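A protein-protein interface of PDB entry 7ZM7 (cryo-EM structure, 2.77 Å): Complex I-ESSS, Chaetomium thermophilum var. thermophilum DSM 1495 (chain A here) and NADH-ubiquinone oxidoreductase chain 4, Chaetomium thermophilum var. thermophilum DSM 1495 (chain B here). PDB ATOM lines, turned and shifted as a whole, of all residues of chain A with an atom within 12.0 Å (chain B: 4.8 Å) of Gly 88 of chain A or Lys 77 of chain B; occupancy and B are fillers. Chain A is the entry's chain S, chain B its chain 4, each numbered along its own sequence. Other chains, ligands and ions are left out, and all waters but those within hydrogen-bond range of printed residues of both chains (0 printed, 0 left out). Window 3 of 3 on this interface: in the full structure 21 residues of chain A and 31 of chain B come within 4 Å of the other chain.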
ATOM      1  N   TYR A  84      16.330  22.506   0.995  1.00  0.00           N
ATOM      2  CA  TYR A  84      16.833  21.928  -0.275  1.00  0.00           C
ATOM      3  C   TYR A  84      16.173  22.655  -1.441  1.00  0.00           C
ATOM      4  O   TYR A  84      14.935  22.658  -1.532  1.00  0.00           O
ATOM      5  CB  TYR A  84      16.515  20.436  -0.377  1.00  0.00           C
ATOM      6  CG  TYR A  84      17.110  19.770  -1.589  1.00  0.00           C
ATOM      7  CD1 TYR A  84      18.462  19.473  -1.654  1.00  0.00           C
ATOM      8  CD2 TYR A  84      16.325  19.448  -2.680  1.00  0.00           C
ATOM      9  CE1 TYR A  84      19.018  18.866  -2.768  1.00  0.00           C
ATOM     10  CE2 TYR A  84      16.866  18.842  -3.799  1.00  0.00           C
ATOM     11  CZ  TYR A  84      18.215  18.551  -3.848  1.00  0.00           C
ATOM     12  OH  TYR A  84      18.745  17.951  -4.954  1.00  0.00           O
ATOM     13  N   GLN A  85      16.986  23.243  -2.314  1.00  0.00           N
ATOM     14  CA  GLN A  85      16.419  23.904  -3.512  1.00  0.00           C
ATOM     15  C   GLN A  85      16.174  22.820  -4.559  1.00  0.00           C
ATOM     16  O   GLN A  85      17.128  22.092  -4.894  1.00  0.00           O
ATOM     17  CB  GLN A  85      17.367  24.994  -4.013  1.00  0.00           C
ATOM     18  CG  GLN A  85      17.729  26.011  -2.940  1.00  0.00           C
ATOM     19  CD  GLN A  85      16.510  26.664  -2.336  1.00  0.00           C
ATOM     20  OE1 GLN A  85      16.316  26.658  -1.122  1.00  0.00           O
ATOM     21  NE2 GLN A  85      15.669  27.230  -3.186  1.00  0.00           N
ATOM     22  N   ASN A  86      14.974  22.754  -5.136  1.00  0.00           N
ATOM     23  CA  ASN A  86      14.700  21.760  -6.213  1.00  0.00           C
ATOM     24  C   ASN A  86      15.496  22.067  -7.485  1.00  0.00           C
ATOM     25  O   ASN A  86      15.318  23.161  -8.038  1.00  0.00           O
ATOM     26  CB  ASN A  86      13.207  21.568  -6.486  1.00  0.00           C
ATOM     27  CG  ASN A  86      12.599  20.446  -5.673  1.00  0.00           C
ATOM     28  OD1 ASN A  86      11.582  19.876  -6.057  1.00  0.00           O
ATOM     29  ND2 ASN A  86      13.225  20.109  -4.556  1.00  0.00           N
ATOM     30  N   GLU A  87      16.328  21.125  -7.931  1.00  0.00           N
ATOM     31  CA  GLU A  87      17.138  21.259  -9.179  1.00  0.00           C
ATOM     32  C   GLU A  87      16.315  21.161 -10.479  1.00  0.00           C
ATOM     33  O   GLU A  87      16.644  21.905 -11.419  1.00  0.00           O
ATOM     34  CB  GLU A  87      18.243  20.207  -9.161  1.00  0.00           C
ATOM     35  CG  GLU A  87      19.054  20.208  -7.878  1.00  0.00           C
ATOM     36  CD  GLU A  87      20.168  19.179  -7.840  1.00  0.00           C
ATOM     37  OE1 GLU A  87      20.937  19.180  -6.861  1.00  0.00           O
ATOM     38  OE2 GLU A  87      20.263  18.377  -8.787  1.00  0.00           O
ATOM     39  N   GLY A  88      15.326  20.265 -10.560  1.00  0.00           N
ATOM     40  CA  GLY A  88      14.548  20.053 -11.802  1.00  0.00           C
ATOM     41  C   GLY A  88      14.145  18.596 -11.927  1.00  0.00           C
ATOM     42  O   GLY A  88      12.931  18.348 -12.027  1.00  0.00           O
ATOM     43  N   TRP A  89      15.111  17.673 -11.975  1.00  0.00           N
ATOM     44  CA  TRP A  89      14.852  16.205 -11.939  1.00  0.00           C
ATOM     45  C   TRP A  89      13.802  15.765 -10.916  1.00  0.00           C
ATOM     46  O   TRP A  89      13.016  14.888 -11.270  1.00  0.00           O
ATOM     47  CB  TRP A  89      16.179  15.466 -11.713  1.00  0.00           C
ATOM     48  CG  TRP A  89      16.723  15.603 -10.325  1.00  0.00           C
ATOM     49  CD1 TRP A  89      17.571  16.566  -9.862  1.00  0.00           C
ATOM     50  CD2 TRP A  89      16.439  14.751  -9.202  1.00  0.00           C
ATOM     51  NE1 TRP A  89      17.832  16.372  -8.533  1.00  0.00           N
ATOM     52  CE2 TRP A  89      17.149  15.268  -8.100  1.00  0.00           C
ATOM     53  CE3 TRP A  89      15.653  13.609  -9.019  1.00  0.00           C
ATOM     54  CZ2 TRP A  89      17.081  14.686  -6.836  1.00  0.00           C
ATOM     55  CZ3 TRP A  89      15.594  13.031  -7.772  1.00  0.00           C
ATOM     56  CH2 TRP A  89      16.305  13.561  -6.698  1.00  0.00           C
ATOM     57  N   GLU A  90      13.794  16.318  -9.703  1.00  0.00           N
ATOM     58  CA  GLU A  90      12.893  15.842  -8.613  1.00  0.00           C
ATOM     59  C   GLU A  90      11.469  15.685  -9.132  1.00  0.00           C
ATOM     60  O   GLU A  90      10.879  14.624  -8.885  1.00  0.00           O
ATOM     61  CB  GLU A  90      12.925  16.800  -7.424  1.00  0.00           C
ATOM     62  CG  GLU A  90      14.242  16.859  -6.678  1.00  0.00           C
ATOM     63  CD  GLU A  90      15.257  17.823  -7.261  1.00  0.00           C
ATOM     64  OE1 GLU A  90      15.135  18.156  -8.438  1.00  0.00           O
ATOM     65  OE2 GLU A  90      16.173  18.226  -6.542  1.00  0.00           O
ATOM     66  N   GLY A  91      10.951  16.706  -9.817  1.00  0.00           N
ATOM     67  CA  GLY A  91       9.578  16.671 -10.346  1.00  0.00           C
ATOM     68  C   GLY A  91       9.273  15.370 -11.076  1.00  0.00           C
ATOM     69  O   GLY A  91       8.465  14.597 -10.534  1.00  0.00           O
ATOM     70  N   PRO A  92       9.824  15.070 -12.283  1.00  0.00           N
ATOM     71  CA  PRO A  92       9.433  13.857 -13.012  1.00  0.00           C
ATOM     72  C   PRO A  92       9.973  12.571 -12.412  1.00  0.00           C
ATOM     73  O   PRO A  92       9.345  11.521 -12.578  1.00  0.00           O
ATOM     74  CB  PRO A  92       9.998  14.096 -14.417  1.00  0.00           C
ATOM     75  CG  PRO A  92      10.383  15.537 -14.453  1.00  0.00           C
ATOM     76  CD  PRO A  92      10.730  15.909 -13.078  1.00  0.00           C
ATOM     77  N   PHE A  93      11.114  12.610 -11.729  1.00  0.00           N
ATOM     78  CA  PHE A  93      11.717  11.377 -11.236  1.00  0.00           C
ATOM     79  C   PHE A  93      10.905  10.772 -10.105  1.00  0.00           C
ATOM     80  O   PHE A  93      10.902   9.555  -9.923  1.00  0.00           O
ATOM     81  CB  PHE A  93      13.152  11.655 -10.804  1.00  0.00           C
ATOM     82  CG  PHE A  93      13.907  10.444 -10.336  1.00  0.00           C
ATOM     83  CD1 PHE A  93      13.777   9.961  -9.048  1.00  0.00           C
ATOM     84  CD2 PHE A  93      14.750   9.780 -11.200  1.00  0.00           C
ATOM     85  CE1 PHE A  93      14.466   8.852  -8.645  1.00  0.00           C
ATOM     86  CE2 PHE A  93      15.435   8.679 -10.793  1.00  0.00           C
ATOM     87  CZ  PHE A  93      15.296   8.222  -9.509  1.00  0.00           C
ATOM     88  N   PHE A  94      10.222  11.597  -9.332  1.00  0.00           N
ATOM     89  CA  PHE A  94       9.484  11.110  -8.181  1.00  0.00           C
ATOM     90  C   PHE A  94       8.045  10.760  -8.524  1.00  0.00           C
ATOM     91  O   PHE A  94       7.478   9.828  -7.952  1.00  0.00           O
ATOM     92  CB  PHE A  94       9.541  12.156  -7.073  1.00  0.00           C
ATOM     93  CG  PHE A  94      10.838  12.178  -6.339  1.00  0.00           C
ATOM     94  CD1 PHE A  94      11.801  11.235  -6.585  1.00  0.00           C
ATOM     95  CD2 PHE A  94      11.103  13.157  -5.414  1.00  0.00           C
ATOM     96  CE1 PHE A  94      12.991  11.261  -5.910  1.00  0.00           C
ATOM     97  CE2 PHE A  94      12.294  13.185  -4.743  1.00  0.00           C
ATOM     98  CZ  PHE A  94      13.234  12.240  -4.990  1.00  0.00           C
ATOM     99  N   TYR A  95       7.443  11.495  -9.446  1.00  0.00           N
ATOM    100  CA  TYR A  95       6.073  11.241  -9.852  1.00  0.00           C
ATOM    101  C   TYR A  95       5.998  10.310 -11.046  1.00  0.00           C
ATOM    102  O   TYR A  95       5.180   9.388 -11.062  1.00  0.00           O
ATOM    103  CB  TYR A  95       5.376  12.552 -10.193  1.00  0.00           C
ATOM    104  CG  TYR A  95       5.168  13.452  -9.016  1.00  0.00           C
ATOM    105  CD1 TYR A  95       4.681  12.952  -7.819  1.00  0.00           C
ATOM    106  CD2 TYR A  95       5.444  14.803  -9.100  1.00  0.00           C
ATOM    107  CE1 TYR A  95       4.482  13.774  -6.734  1.00  0.00           C
ATOM    108  CE2 TYR A  95       5.247  15.635  -8.021  1.00  0.00           C
ATOM    109  CZ  TYR A  95       4.767  15.115  -6.841  1.00  0.00           C
ATOM    110  OH  TYR A  95       4.571  15.941  -5.762  1.00  0.00           O
ATOM    111  N   GLY A  96       6.837  10.537 -12.046  1.00  0.00           N
ATOM    112  CA  GLY A  96       6.778   9.756 -13.255  1.00  0.00           C
ATOM    113  C   GLY A  96       7.573   8.484 -13.158  1.00  0.00           C
ATOM    114  O   GLY A  96       7.045   7.411 -13.436  1.00  0.00           O
ATOM    115  N   PHE A  97       8.845   8.585 -12.772  1.00  0.00           N
ATOM    116  CA  PHE A  97       9.703   7.409 -12.747  1.00  0.00           C
ATOM    117  C   PHE A  97       9.222   6.454 -11.674  1.00  0.00           C
ATOM    118  O   PHE A  97       8.784   5.352 -11.985  1.00  0.00           O
ATOM    119  CB  PHE A  97      11.165   7.788 -12.524  1.00  0.00           C
ATOM    120  CG  PHE A  97      12.116   6.639 -12.669  1.00  0.00           C
ATOM    121  CD1 PHE A  97      12.588   6.268 -13.911  1.00  0.00           C
ATOM    122  CD2 PHE A  97      12.531   5.920 -11.567  1.00  0.00           C
ATOM    123  CE1 PHE A  97      13.466   5.208 -14.045  1.00  0.00           C
ATOM    124  CE2 PHE A  97      13.392   4.868 -11.701  1.00  0.00           C
ATOM    125  CZ  PHE A  97      13.856   4.511 -12.940  1.00  0.00           C
ATOM    126  N   SER B  73      17.875  24.371 -18.305  1.00  0.00           N
ATOM    127  CA  SER B  73      17.102  23.554 -17.381  1.00  0.00           C
ATOM    128  C   SER B  73      15.873  22.989 -18.065  1.00  0.00           C
ATOM    129  O   SER B  73      15.461  21.857 -17.791  1.00  0.00           O
ATOM    130  CB  SER B  73      16.705  24.375 -16.156  1.00  0.00           C
ATOM    131  OG  SER B  73      15.978  23.591 -15.225  1.00  0.00           O
ATOM    132  N   TYR B  74      15.274  23.765 -18.955  1.00  0.00           N
ATOM    133  CA  TYR B  74      14.105  23.310 -19.677  1.00  0.00           C
ATOM    134  C   TYR B  74      14.468  22.361 -20.811  1.00  0.00           C
ATOM    135  O   TYR B  74      13.616  21.599 -21.262  1.00  0.00           O
ATOM    136  CB  TYR B  74      13.317  24.532 -20.161  1.00  0.00           C
ATOM    137  CG  TYR B  74      12.047  24.197 -20.884  1.00  0.00           C
ATOM    138  CD1 TYR B  74      10.934  23.768 -20.184  1.00  0.00           C
ATOM    139  CD2 TYR B  74      11.934  24.359 -22.256  1.00  0.00           C
ATOM    140  CE1 TYR B  74       9.753  23.455 -20.831  1.00  0.00           C
ATOM    141  CE2 TYR B  74      10.750  24.063 -22.915  1.00  0.00           C
ATOM    142  CZ  TYR B  74       9.663  23.607 -22.193  1.00  0.00           C
ATOM    143  OH  TYR B  74       8.481  23.308 -22.832  1.00  0.00           O
ATOM    144  N   TYR B  75      15.722  22.379 -21.259  1.00  0.00           N
ATOM    145  CA  TYR B  75      16.222  21.356 -22.168  1.00  0.00           C
ATOM    146  C   TYR B  75      16.274  20.011 -21.469  1.00  0.00           C
ATOM    147  O   TYR B  75      15.933  18.977 -22.049  1.00  0.00           O
ATOM    148  CB  TYR B  75      17.624  21.736 -22.634  1.00  0.00           C
ATOM    149  CG  TYR B  75      17.683  22.772 -23.704  1.00  0.00           C
ATOM    150  CD1 TYR B  75      16.622  22.984 -24.558  1.00  0.00           C
ATOM    151  CD2 TYR B  75      18.759  23.638 -23.770  1.00  0.00           C
ATOM    152  CE1 TYR B  75      16.669  23.976 -25.496  1.00  0.00           C
ATOM    153  CE2 TYR B  75      18.813  24.635 -24.690  1.00  0.00           C
ATOM    154  CZ  TYR B  75      17.767  24.801 -25.556  1.00  0.00           C
ATOM    155  OH  TYR B  75      17.824  25.795 -26.501  1.00  0.00           O
ATOM    156  N   LYS B  76      16.730  20.012 -20.215  1.00  0.00           N
ATOM    157  CA  LYS B  76      16.939  18.777 -19.473  1.00  0.00           C
ATOM    158  C   LYS B  76      15.626  18.154 -19.050  1.00  0.00           C
ATOM    159  O   LYS B  76      15.519  16.930 -18.960  1.00  0.00           O
ATOM    160  CB  LYS B  76      17.783  19.036 -18.238  1.00  0.00           C
ATOM    161  CG  LYS B  76      19.061  19.737 -18.459  1.00  0.00           C
ATOM    162  CD  LYS B  76      19.599  20.201 -17.130  1.00  0.00           C
ATOM    163  CE  LYS B  76      20.979  20.742 -17.247  1.00  0.00           C
ATOM    164  NZ  LYS B  76      21.929  19.686 -16.870  1.00  0.00           N
ATOM    165  N   LYS B  77      14.640  18.980 -18.719  1.00  0.00           N
ATOM    166  CA  LYS B  77      13.365  18.453 -18.257  1.00  0.00           C
ATOM    167  C   LYS B  77      12.636  17.743 -19.382  1.00  0.00           C
ATOM    168  O   LYS B  77      11.990  16.718 -19.161  1.00  0.00           O
ATOM    169  CB  LYS B  77      12.513  19.578 -17.682  1.00  0.00           C
ATOM    170  CG  LYS B  77      13.053  20.164 -16.407  1.00  0.00           C
ATOM    171  CD  LYS B  77      12.147  21.254 -15.872  1.00  0.00           C
ATOM    172  CE  LYS B  77      12.705  21.855 -14.610  1.00  0.00           C
ATOM    173  NZ  LYS B  77      11.847  22.926 -14.079  1.00  0.00           N
ATOM    174  N   ILE B  78      12.724  18.278 -20.596  1.00  0.00           N
ATOM    175  CA  ILE B  78      12.049  17.655 -21.722  1.00  0.00           C
ATOM    176  C   ILE B  78      12.645  16.288 -22.006  1.00  0.00           C
ATOM    177  O   ILE B  78      11.917  15.317 -22.235  1.00  0.00           O
ATOM    178  CB  ILE B  78      12.119  18.567 -22.951  1.00  0.00           C
ATOM    179  CG1 ILE B  78      11.313  19.826 -22.705  1.00  0.00           C
ATOM    180  CG2 ILE B  78      11.582  17.849 -24.168  1.00  0.00           C
ATOM    181  CD1 ILE B  78      11.571  20.866 -23.704  1.00  0.00           C
ATOM    182  N   ALA B  79      13.970  16.183 -21.987  1.00  0.00           N
ATOM    183  CA  ALA B  79      14.601  14.912 -22.296  1.00  0.00           C
ATOM    184  C   ALA B  79      14.299  13.878 -21.226  1.00  0.00           C
ATOM    185  O   ALA B  79      14.153  12.690 -21.524  1.00  0.00           O
ATOM    186  CB  ALA B  79      16.108  15.098 -22.466  1.00  0.00           C
ATOM    187  N   LEU B  80      14.215  14.302 -19.972  1.00  0.00           N
ATOM    188  CA  LEU B  80      13.954  13.351 -18.904  1.00  0.00           C
ATOM    189  C   LEU B  80      12.502  12.908 -18.885  1.00  0.00           C
ATOM    190  O   LEU B  80      12.218  11.731 -18.664  1.00  0.00           O
ATOM    191  CB  LEU B  80      14.360  13.945 -17.567  1.00  0.00           C
ATOM    192  CG  LEU B  80      13.976  13.119 -16.355  1.00  0.00           C
ATOM    193  CD1 LEU B  80      14.990  12.014 -16.117  1.00  0.00           C
ATOM    194  CD2 LEU B  80      13.857  14.025 -15.161  1.00  0.00           C
ATOM    195  N   ILE B  81      11.569  13.829 -19.121  1.00  0.00           N
ATOM    196  CA  ILE B  81      10.167  13.439 -19.222  1.00  0.00           C
ATOM    197  C   ILE B  81       9.979  12.448 -20.354  1.00  0.00           C
ATOM    198  O   ILE B  81       9.211  11.490 -20.240  1.00  0.00           O
ATOM    199  CB  ILE B  81       9.269  14.672 -19.414  1.00  0.00           C
ATOM    200  CG1 ILE B  81       8.964  15.332 -18.082  1.00  0.00           C
ATOM    201  CG2 ILE B  81       7.974  14.288 -20.076  1.00  0.00           C
ATOM    202  CD1 ILE B  81       8.359  16.679 -18.249  1.00  0.00           C
ATOM    203  N   TRP B 145      23.282  15.098 -14.523  1.00  0.00           N
ATOM    204  CA  TRP B 145      22.444  16.328 -14.580  1.00  0.00           C
ATOM    205  C   TRP B 145      23.224  17.625 -14.411  1.00  0.00           C
ATOM    206  O   TRP B 145      22.795  18.612 -14.970  1.00  0.00           O
ATOM    207  CB  TRP B 145      21.359  16.228 -13.504  1.00  0.00           C
ATOM    208  CG  TRP B 145      20.224  17.200 -13.619  1.00  0.00           C
ATOM    209  CD1 TRP B 145      20.138  18.437 -13.050  1.00  0.00           C
ATOM    210  CD2 TRP B 145      18.982  16.995 -14.314  1.00  0.00           C
ATOM    211  NE1 TRP B 145      18.942  19.024 -13.361  1.00  0.00           N
ATOM    212  CE2 TRP B 145      18.210  18.163 -14.134  1.00  0.00           C
ATOM    213  CE3 TRP B 145      18.452  15.947 -15.074  1.00  0.00           C
ATOM    214  CZ2 TRP B 145      16.942  18.307 -14.691  1.00  0.00           C
ATOM    215  CZ3 TRP B 145      17.198  16.092 -15.623  1.00  0.00           C
ATOM    216  CH2 TRP B 145      16.454  17.255 -15.429  1.00  0.00           C
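NE1 of Trp 89 of chain A lies within hydrogen-bond range of OE2 of Glu 90 of chain A.
The backbone carbonyl oxygen (O) of Pro 92 of chain A is in hydrogen-bond range of the backbone NH (N) of Phe 97 of chain A.
The backbone NH of Gly 88 of chain A lies within hydrogen-bond range of the side-chain carboxylate of Glu 90 of chain A.
The indole nitrogen (NE1) of Trp 89 of chain A is in hydrogen-bond range of the side-chain carboxylate (OE2) of Glu 87 of chain A, 3.2 Å away.
Among the printed residues, pairs that only touch across the chains: Trp 89 of chain A with Trp 145 of chain B (3.3 Å), Gly 88 of chain A with Lys 77 of chain B (3.8 Å), Pro 92 of chain A with Leu 80 of chain B (3.9 Å), Pro 92 of chain A with Ile 81 of chain B (3.9 Å) and Gly 88 of chain A with Trp 145 of chain B (3.9 Å).
Glu 87 of chain A touches none of the printed residues of chain B.
Gly 88 of chain A touches two residues of chain B.
Of the printed residues of chain B, Trp 89 of chain A touches Trp 145 (3.3 Å).
Printed residues of chain B within 4 Å of Pro 92 of chain A: Leu 80 (3.9 Å) and Ile 81 (3.9 Å).
No residue of chain A comes within 4 Å of Ser 73 of chain B.
Lys 76 of chain B touches none of the printed residues of chain A.
Of the printed residues of chain A, Lys 77 of chain B touches Gly 88 (3.8 Å).
No residue of chain A comes within 4 Å of Ile 78 of chain B.
No residue of chain A comes within 4 Å of Ala 79 of chain B.
Of the printed residues of chain A, Leu 80 of chain B touches Pro 92 (3.9 Å).
Of chain A, only Pro 92 comes within 4 Å of Ile 81 of chain B.
Printed residues of chain A within 4 Å of Trp 145 of chain B: Gly 88 (3.9 Å) and Trp 89 (3.3 Å).
The nearest residue of chain A that does not touch Lys 77 of chain B is Glu 87 of chain A (5.1 Å).
The nearest printed residue of chain A that does not touch Trp 145 of chain B is Glu 87 of chain A (4.2 Å).
Of the 14 printed residues of chain A, 3 touch a printed residue of chain B.
Hydrophobic or aromatic side chains of chain A that line the printed part of chain B: Pro 92.
Among the printed residues, 5 pairs touch across the chains.
Among the printed residues, no Asp or Glu carboxylate lies within 4 Å of a Lys or Arg side-chain nitrogen of the other chain.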
